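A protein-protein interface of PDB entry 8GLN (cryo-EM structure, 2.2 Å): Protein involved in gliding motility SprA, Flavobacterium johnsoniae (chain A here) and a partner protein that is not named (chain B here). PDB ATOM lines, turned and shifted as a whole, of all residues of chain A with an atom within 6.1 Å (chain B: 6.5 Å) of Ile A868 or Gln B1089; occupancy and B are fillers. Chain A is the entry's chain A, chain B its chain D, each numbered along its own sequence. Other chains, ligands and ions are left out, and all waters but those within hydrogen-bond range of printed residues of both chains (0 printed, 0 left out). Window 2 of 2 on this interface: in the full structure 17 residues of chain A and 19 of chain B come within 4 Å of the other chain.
Among the printed residues, pairs that only touch across the chains: Thr A867 with Gln B1089, Ile A868 with Gln B1089, Asp A869 with Lys B1048 and Arg A1261 with Asn B1087.
Of the 12 printed residues of chain A, 4 touch a printed residue of chain B. Of the 11 printed residues of chain B, 3 touch a printed residue of chain A. Printed residues of chain B that touch a printed residue of chain A: Lys B1048, Asn B1087 and Gln B1089. Along chain B the printed residues that touch a printed residue of chain A span positions 1048 to 1089. Among the printed residues, no Asp or Glu carboxylate lies within 4 Å of a Lys or Arg side-chain nitrogen of the other chain.
The side-chain hydroxyl (OG) of Ser A866 lies within hydrogen-bond range of the guanidinium group (NH1) of Arg A1261 (2.9 Å). N of Ile A868 lies within hydrogen-bond range of O of Leu A1259 (2.8 Å).
The backbone NH (N) of Asp A869 is in hydrogen-bond range of the side-chain amide oxygen (OE1) of Gln B1089 (2.5 Å).
Printed residues of chain B within 4 Å of Asp A869: Lys B1048 and Gln B1089. Ser A996 touches none of the printed residues of chain B. Of the printed residues of chain B, Arg A1261 touches Asn B1087 (3.6 Å). Of the printed residues of chain A, Lys B1048 touches Asp A869 (3.8 Å). Of the printed residues of chain A, Asn B1087 touches Arg A1261. Gln B1089 touches just these residues of chain A: Thr A867, Ile A868 and Asp A869. The nearest printed residue of chain A that does not touch Lys B1048 is Met A870 (5.5 Å).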
ATOM      1  N   SER A 866      23.624 -14.339   0.135  1.00  0.00           N
ATOM      2  CA  SER A 866      22.349 -13.947   0.719  1.00  0.00           C
ATOM      3  C   SER A 866      21.279 -13.874  -0.367  1.00  0.00           C
ATOM      4  O   SER A 866      21.560 -13.559  -1.527  1.00  0.00           O
ATOM      5  CB  SER A 866      22.474 -12.603   1.435  1.00  0.00           C
ATOM      6  OG  SER A 866      22.657 -11.548   0.510  1.00  0.00           O
ATOM      7  N   THR A 867      20.040 -14.168   0.016  1.00  0.00           N
ATOM      8  CA  THR A 867      18.950 -14.330  -0.936  1.00  0.00           C
ATOM      9  C   THR A 867      17.848 -13.308  -0.690  1.00  0.00           C
ATOM     10  O   THR A 867      17.632 -12.856   0.438  1.00  0.00           O
ATOM     11  CB  THR A 867      18.351 -15.742  -0.866  1.00  0.00           C
ATOM     12  OG1 THR A 867      17.797 -15.963   0.436  1.00  0.00           O
ATOM     13  CG2 THR A 867      19.417 -16.790  -1.142  1.00  0.00           C
ATOM     14  N   ILE A 868      17.152 -12.952  -1.767  1.00  0.00           N
ATOM     15  CA  ILE A 868      15.999 -12.059  -1.723  1.00  0.00           C
ATOM     16  C   ILE A 868      14.786 -12.865  -2.162  1.00  0.00           C
ATOM     17  O   ILE A 868      14.665 -13.223  -3.341  1.00  0.00           O
ATOM     18  CB  ILE A 868      16.195 -10.825  -2.614  1.00  0.00           C
ATOM     19  CG1 ILE A 868      17.521 -10.138  -2.289  1.00  0.00           C
ATOM     20  CG2 ILE A 868      15.026  -9.864  -2.457  1.00  0.00           C
ATOM     21  CD1 ILE A 868      18.045  -9.268  -3.406  1.00  0.00           C
ATOM     22  N   ASP A 869      13.883 -13.142  -1.225  1.00  0.00           N
ATOM     23  CA  ASP A 869      12.718 -13.968  -1.519  1.00  0.00           C
ATOM     24  C   ASP A 869      11.798 -13.267  -2.513  1.00  0.00           C
ATOM     25  O   ASP A 869      11.507 -12.076  -2.373  1.00  0.00           O
ATOM     26  CB  ASP A 869      11.963 -14.286  -0.230  1.00  0.00           C
ATOM     27  CG  ASP A 869      10.996 -15.440  -0.390  1.00  0.00           C
ATOM     28  OD1 ASP A 869      11.013 -16.093  -1.454  1.00  0.00           O
ATOM     29  OD2 ASP A 869      10.218 -15.696   0.552  1.00  0.00           O
ATOM     30  N   MET A 870      11.332 -14.015  -3.513  1.00  0.00           N
ATOM     31  CA  MET A 870      10.512 -13.471  -4.590  1.00  0.00           C
ATOM     32  C   MET A 870       9.175 -14.182  -4.750  1.00  0.00           C
ATOM     33  O   MET A 870       8.498 -13.970  -5.761  1.00  0.00           O
ATOM     34  CB  MET A 870      11.274 -13.527  -5.918  1.00  0.00           C
ATOM     35  CG  MET A 870      12.533 -12.679  -5.986  1.00  0.00           C
ATOM     36  SD  MET A 870      12.216 -10.981  -6.498  1.00  0.00           S
ATOM     37  CE  MET A 870      12.014 -10.165  -4.921  1.00  0.00           C
ATOM     38  N   SER A 996      15.638  -3.587  -4.381  1.00  0.00           N
ATOM     39  CA  SER A 996      17.005  -3.143  -4.636  1.00  0.00           C
ATOM     40  C   SER A 996      17.266  -3.232  -6.135  1.00  0.00           C
ATOM     41  O   SER A 996      17.282  -4.326  -6.706  1.00  0.00           O
ATOM     42  CB  SER A 996      18.009  -3.982  -3.849  1.00  0.00           C
ATOM     43  OG  SER A 996      17.560  -4.202  -2.525  1.00  0.00           O
ATOM     44  N   VAL A1004      24.167  -9.079  -7.411  1.00  0.00           N
ATOM     45  CA  VAL A1004      23.187 -10.119  -7.707  1.00  0.00           C
ATOM     46  C   VAL A1004      23.758 -11.015  -8.797  1.00  0.00           C
ATOM     47  O   VAL A1004      24.116 -10.543  -9.882  1.00  0.00           O
ATOM     48  CB  VAL A1004      21.844  -9.512  -8.129  1.00  0.00           C
ATOM     49  CG1 VAL A1004      20.908 -10.600  -8.638  1.00  0.00           C
ATOM     50  CG2 VAL A1004      21.215  -8.759  -6.968  1.00  0.00           C
ATOM     51  N   LEU A1257      12.105 -19.292  -4.608  1.00  0.00           N
ATOM     52  CA  LEU A1257      12.356 -18.437  -5.767  1.00  0.00           C
ATOM     53  C   LEU A1257      13.031 -17.176  -5.250  1.00  0.00           C
ATOM     54  O   LEU A1257      12.369 -16.331  -4.641  1.00  0.00           O
ATOM     55  CB  LEU A1257      11.061 -18.114  -6.506  1.00  0.00           C
ATOM     56  CG  LEU A1257      11.152 -17.131  -7.674  1.00  0.00           C
ATOM     57  CD1 LEU A1257      11.990 -17.697  -8.811  1.00  0.00           C
ATOM     58  CD2 LEU A1257       9.766 -16.753  -8.171  1.00  0.00           C
ATOM     59  N   ASP A1258      14.334 -17.053  -5.484  1.00  0.00           N
ATOM     60  CA  ASP A1258      15.112 -15.971  -4.905  1.00  0.00           C
ATOM     61  C   ASP A1258      16.053 -15.370  -5.935  1.00  0.00           C
ATOM     62  O   ASP A1258      16.488 -16.039  -6.876  1.00  0.00           O
ATOM     63  CB  ASP A1258      15.949 -16.441  -3.702  1.00  0.00           C
ATOM     64  CG  ASP A1258      15.208 -17.415  -2.812  1.00  0.00           C
ATOM     65  OD1 ASP A1258      14.988 -17.090  -1.627  1.00  0.00           O
ATOM     66  OD2 ASP A1258      14.866 -18.516  -3.291  1.00  0.00           O
ATOM     67  N   LEU A1259      16.355 -14.091  -5.741  1.00  0.00           N
ATOM     68  CA  LEU A1259      17.541 -13.477  -6.314  1.00  0.00           C
ATOM     69  C   LEU A1259      18.679 -13.664  -5.319  1.00  0.00           C
ATOM     70  O   LEU A1259      18.520 -13.373  -4.130  1.00  0.00           O
ATOM     71  CB  LEU A1259      17.306 -11.993  -6.596  1.00  0.00           C
ATOM     72  CG  LEU A1259      16.195 -11.653  -7.593  1.00  0.00           C
ATOM     73  CD1 LEU A1259      16.119 -10.152  -7.817  1.00  0.00           C
ATOM     74  CD2 LEU A1259      16.410 -12.375  -8.908  1.00  0.00           C
ATOM     75  N   VAL A1260      19.813 -14.164  -5.797  1.00  0.00           N
ATOM     76  CA  VAL A1260      20.936 -14.512  -4.934  1.00  0.00           C
ATOM     77  C   VAL A1260      22.088 -13.570  -5.242  1.00  0.00           C
ATOM     78  O   VAL A1260      22.546 -13.487  -6.388  1.00  0.00           O
ATOM     79  CB  VAL A1260      21.360 -15.978  -5.115  1.00  0.00           C
ATOM     80  CG1 VAL A1260      22.568 -16.285  -4.245  1.00  0.00           C
ATOM     81  CG2 VAL A1260      20.202 -16.907  -4.782  1.00  0.00           C
ATOM     82  N   ARG A1261      22.557 -12.863  -4.221  1.00  0.00           N
ATOM     83  CA  ARG A1261      23.725 -12.004  -4.325  1.00  0.00           C
ATOM     84  C   ARG A1261      24.873 -12.609  -3.531  1.00  0.00           C
ATOM     85  O   ARG A1261      24.684 -13.069  -2.402  1.00  0.00           O
ATOM     86  CB  ARG A1261      23.425 -10.594  -3.815  1.00  0.00           C
ATOM     87  CG  ARG A1261      22.678 -10.558  -2.503  1.00  0.00           C
ATOM     88  CD  ARG A1261      21.949  -9.239  -2.318  1.00  0.00           C
ATOM     89  NE  ARG A1261      22.874  -8.134  -2.096  1.00  0.00           N
ATOM     90  CZ  ARG A1261      23.605  -7.970  -1.001  1.00  0.00           C
ATOM     91  NH1 ARG A1261      23.528  -8.813   0.017  1.00  0.00           N
ATOM     92  NH2 ARG A1261      24.427  -6.928  -0.920  1.00  0.00           N
ATOM     93  N   ASP B1047       8.144  -5.451   3.737  1.00  0.00           N
ATOM     94  CA  ASP B1047       8.305  -6.688   2.966  1.00  0.00           C
ATOM     95  C   ASP B1047       9.751  -7.161   3.098  1.00  0.00           C
ATOM     96  O   ASP B1047      10.593  -6.871   2.245  1.00  0.00           O
ATOM     97  CB  ASP B1047       7.897  -6.473   1.506  1.00  0.00           C
ATOM     98  CG  ASP B1047       8.295  -5.103   0.981  1.00  0.00           C
ATOM     99  OD1 ASP B1047       9.454  -4.689   1.188  1.00  0.00           O
ATOM    100  OD2 ASP B1047       7.441  -4.437   0.361  1.00  0.00           O
ATOM    101  N   LYS B1048      10.026  -7.918   4.160  1.00  0.00           N
ATOM    102  CA  LYS B1048      11.365  -8.443   4.433  1.00  0.00           C
ATOM    103  C   LYS B1048      12.422  -7.338   4.456  1.00  0.00           C
ATOM    104  O   LYS B1048      13.617  -7.602   4.306  1.00  0.00           O
ATOM    105  CB  LYS B1048      11.747  -9.531   3.427  1.00  0.00           C
ATOM    106  CG  LYS B1048      10.887 -10.782   3.504  1.00  0.00           C
ATOM    107  CD  LYS B1048       9.737 -10.730   2.510  1.00  0.00           C
ATOM    108  CE  LYS B1048       9.568 -12.059   1.792  1.00  0.00           C
ATOM    109  NZ  LYS B1048       8.489 -12.001   0.768  1.00  0.00           N
ATOM    110  N   THR B1049      11.994  -6.092   4.641  1.00  0.00           N
ATOM    111  CA  THR B1049      12.897  -4.960   4.778  1.00  0.00           C
ATOM    112  C   THR B1049      12.643  -4.274   6.112  1.00  0.00           C
ATOM    113  O   THR B1049      11.495  -4.120   6.537  1.00  0.00           O
ATOM    114  CB  THR B1049      12.744  -3.964   3.612  1.00  0.00           C
ATOM    115  OG1 THR B1049      13.809  -3.005   3.656  1.00  0.00           O
ATOM    116  CG2 THR B1049      11.403  -3.243   3.656  1.00  0.00           C
ATOM    117  N   VAL B1085      17.532  -1.523   6.273  1.00  0.00           N
ATOM    118  CA  VAL B1085      18.325  -2.755   6.144  1.00  0.00           C
ATOM    119  C   VAL B1085      17.730  -3.516   4.966  1.00  0.00           C
ATOM    120  O   VAL B1085      16.899  -4.417   5.107  1.00  0.00           O
ATOM    121  CB  VAL B1085      18.334  -3.572   7.437  1.00  0.00           C
ATOM    122  CG1 VAL B1085      19.532  -4.497   7.467  1.00  0.00           C
ATOM    123  CG2 VAL B1085      18.329  -2.652   8.647  1.00  0.00           C
ATOM    124  N   SER B1086      18.174  -3.147   3.764  1.00  0.00           N
ATOM    125  CA  SER B1086      17.707  -3.790   2.542  1.00  0.00           C
ATOM    126  C   SER B1086      18.559  -4.978   2.123  1.00  0.00           C
ATOM    127  O   SER B1086      18.084  -5.818   1.351  1.00  0.00           O
ATOM    128  CB  SER B1086      17.658  -2.779   1.391  1.00  0.00           C
ATOM    129  OG  SER B1086      16.447  -2.043   1.411  1.00  0.00           O
ATOM    130  N   ASN B1087      19.795  -5.071   2.609  1.00  0.00           N
ATOM    131  CA  ASN B1087      20.686  -6.175   2.287  1.00  0.00           C
ATOM    132  C   ASN B1087      20.576  -7.322   3.285  1.00  0.00           C
ATOM    133  O   ASN B1087      21.531  -8.092   3.440  1.00  0.00           O
ATOM    134  CB  ASN B1087      22.130  -5.675   2.212  1.00  0.00           C
ATOM    135  CG  ASN B1087      22.351  -4.710   1.065  1.00  0.00           C
ATOM    136  OD1 ASN B1087      21.484  -4.540   0.207  1.00  0.00           O
ATOM    137  ND2 ASN B1087      23.514  -4.069   1.045  1.00  0.00           N
ATOM    138  N   PHE B1088      19.439  -7.446   3.964  1.00  0.00           N
ATOM    139  CA  PHE B1088      19.246  -8.468   4.980  1.00  0.00           C
ATOM    140  C   PHE B1088      17.875  -9.100   4.810  1.00  0.00           C
ATOM    141  O   PHE B1088      16.888  -8.402   4.557  1.00  0.00           O
ATOM    142  CB  PHE B1088      19.389  -7.876   6.389  1.00  0.00           C
ATOM    143  CG  PHE B1088      18.819  -8.740   7.474  1.00  0.00           C
ATOM    144  CD1 PHE B1088      19.515  -9.843   7.936  1.00  0.00           C
ATOM    145  CD2 PHE B1088      17.593  -8.441   8.041  1.00  0.00           C
ATOM    146  CE1 PHE B1088      18.995 -10.635   8.934  1.00  0.00           C
ATOM    147  CE2 PHE B1088      17.070  -9.232   9.040  1.00  0.00           C
ATOM    148  CZ  PHE B1088      17.772 -10.329   9.488  1.00  0.00           C
ATOM    149  N   GLN B1089      17.821 -10.422   4.952  1.00  0.00           N
ATOM    150  CA  GLN B1089      16.558 -11.149   4.858  1.00  0.00           C
ATOM    151  C   GLN B1089      16.744 -12.522   5.484  1.00  0.00           C
ATOM    152  O   GLN B1089      17.581 -13.304   5.021  1.00  0.00           O
ATOM    153  CB  GLN B1089      16.111 -11.269   3.403  1.00  0.00           C
ATOM    154  CG  GLN B1089      14.648 -11.612   3.232  1.00  0.00           C
ATOM    155  CD  GLN B1089      14.388 -12.438   1.991  1.00  0.00           C
ATOM    156  OE1 GLN B1089      13.961 -11.916   0.964  1.00  0.00           O
ATOM    157  NE2 GLN B1089      14.643 -13.736   2.081  1.00  0.00           N
ATOM    158  N   SER B1090      15.974 -12.811   6.530  1.00  0.00           N
ATOM    159  CA  SER B1090      16.036 -14.090   7.228  1.00  0.00           C
ATOM    160  C   SER B1090      14.723 -14.854   7.175  1.00  0.00           C
ATOM    161  O   SER B1090      14.712 -16.033   6.800  1.00  0.00           O
ATOM    162  CB  SER B1090      16.459 -13.869   8.689  1.00  0.00           C
ATOM    163  OG  SER B1090      15.347 -13.523   9.495  1.00  0.00           O
ATOM    164  N   GLY B1091      13.614 -14.218   7.542  1.00  0.00           N
ATOM    165  CA  GLY B1091      12.326 -14.881   7.568  1.00  0.00           C
ATOM    166  C   GLY B1091      12.023 -15.663   8.826  1.00  0.00           C
ATOM    167  O   GLY B1091      11.048 -16.425   8.839  1.00  0.00           O
ATOM    168  N   PHE B1113       9.780 -10.245  11.808  1.00  0.00           N
ATOM    169  CA  PHE B1113      10.272 -10.062  10.444  1.00  0.00           C
ATOM    170  C   PHE B1113       9.226 -10.606   9.475  1.00  0.00           C
ATOM    171  O   PHE B1113       9.261 -11.761   9.044  1.00  0.00           O
ATOM    172  CB  PHE B1113      11.620 -10.743  10.264  1.00  0.00           C
ATOM    173  CG  PHE B1113      12.391 -10.245   9.082  1.00  0.00           C
ATOM    174  CD1 PHE B1113      13.226 -11.090   8.375  1.00  0.00           C
ATOM    175  CD2 PHE B1113      12.291  -8.924   8.687  1.00  0.00           C
ATOM    176  CE1 PHE B1113      13.937 -10.627   7.289  1.00  0.00           C
ATOM    177  CE2 PHE B1113      12.999  -8.456   7.604  1.00  0.00           C
ATOM    178  CZ  PHE B1113      13.825  -9.308   6.905  1.00  0.00           C
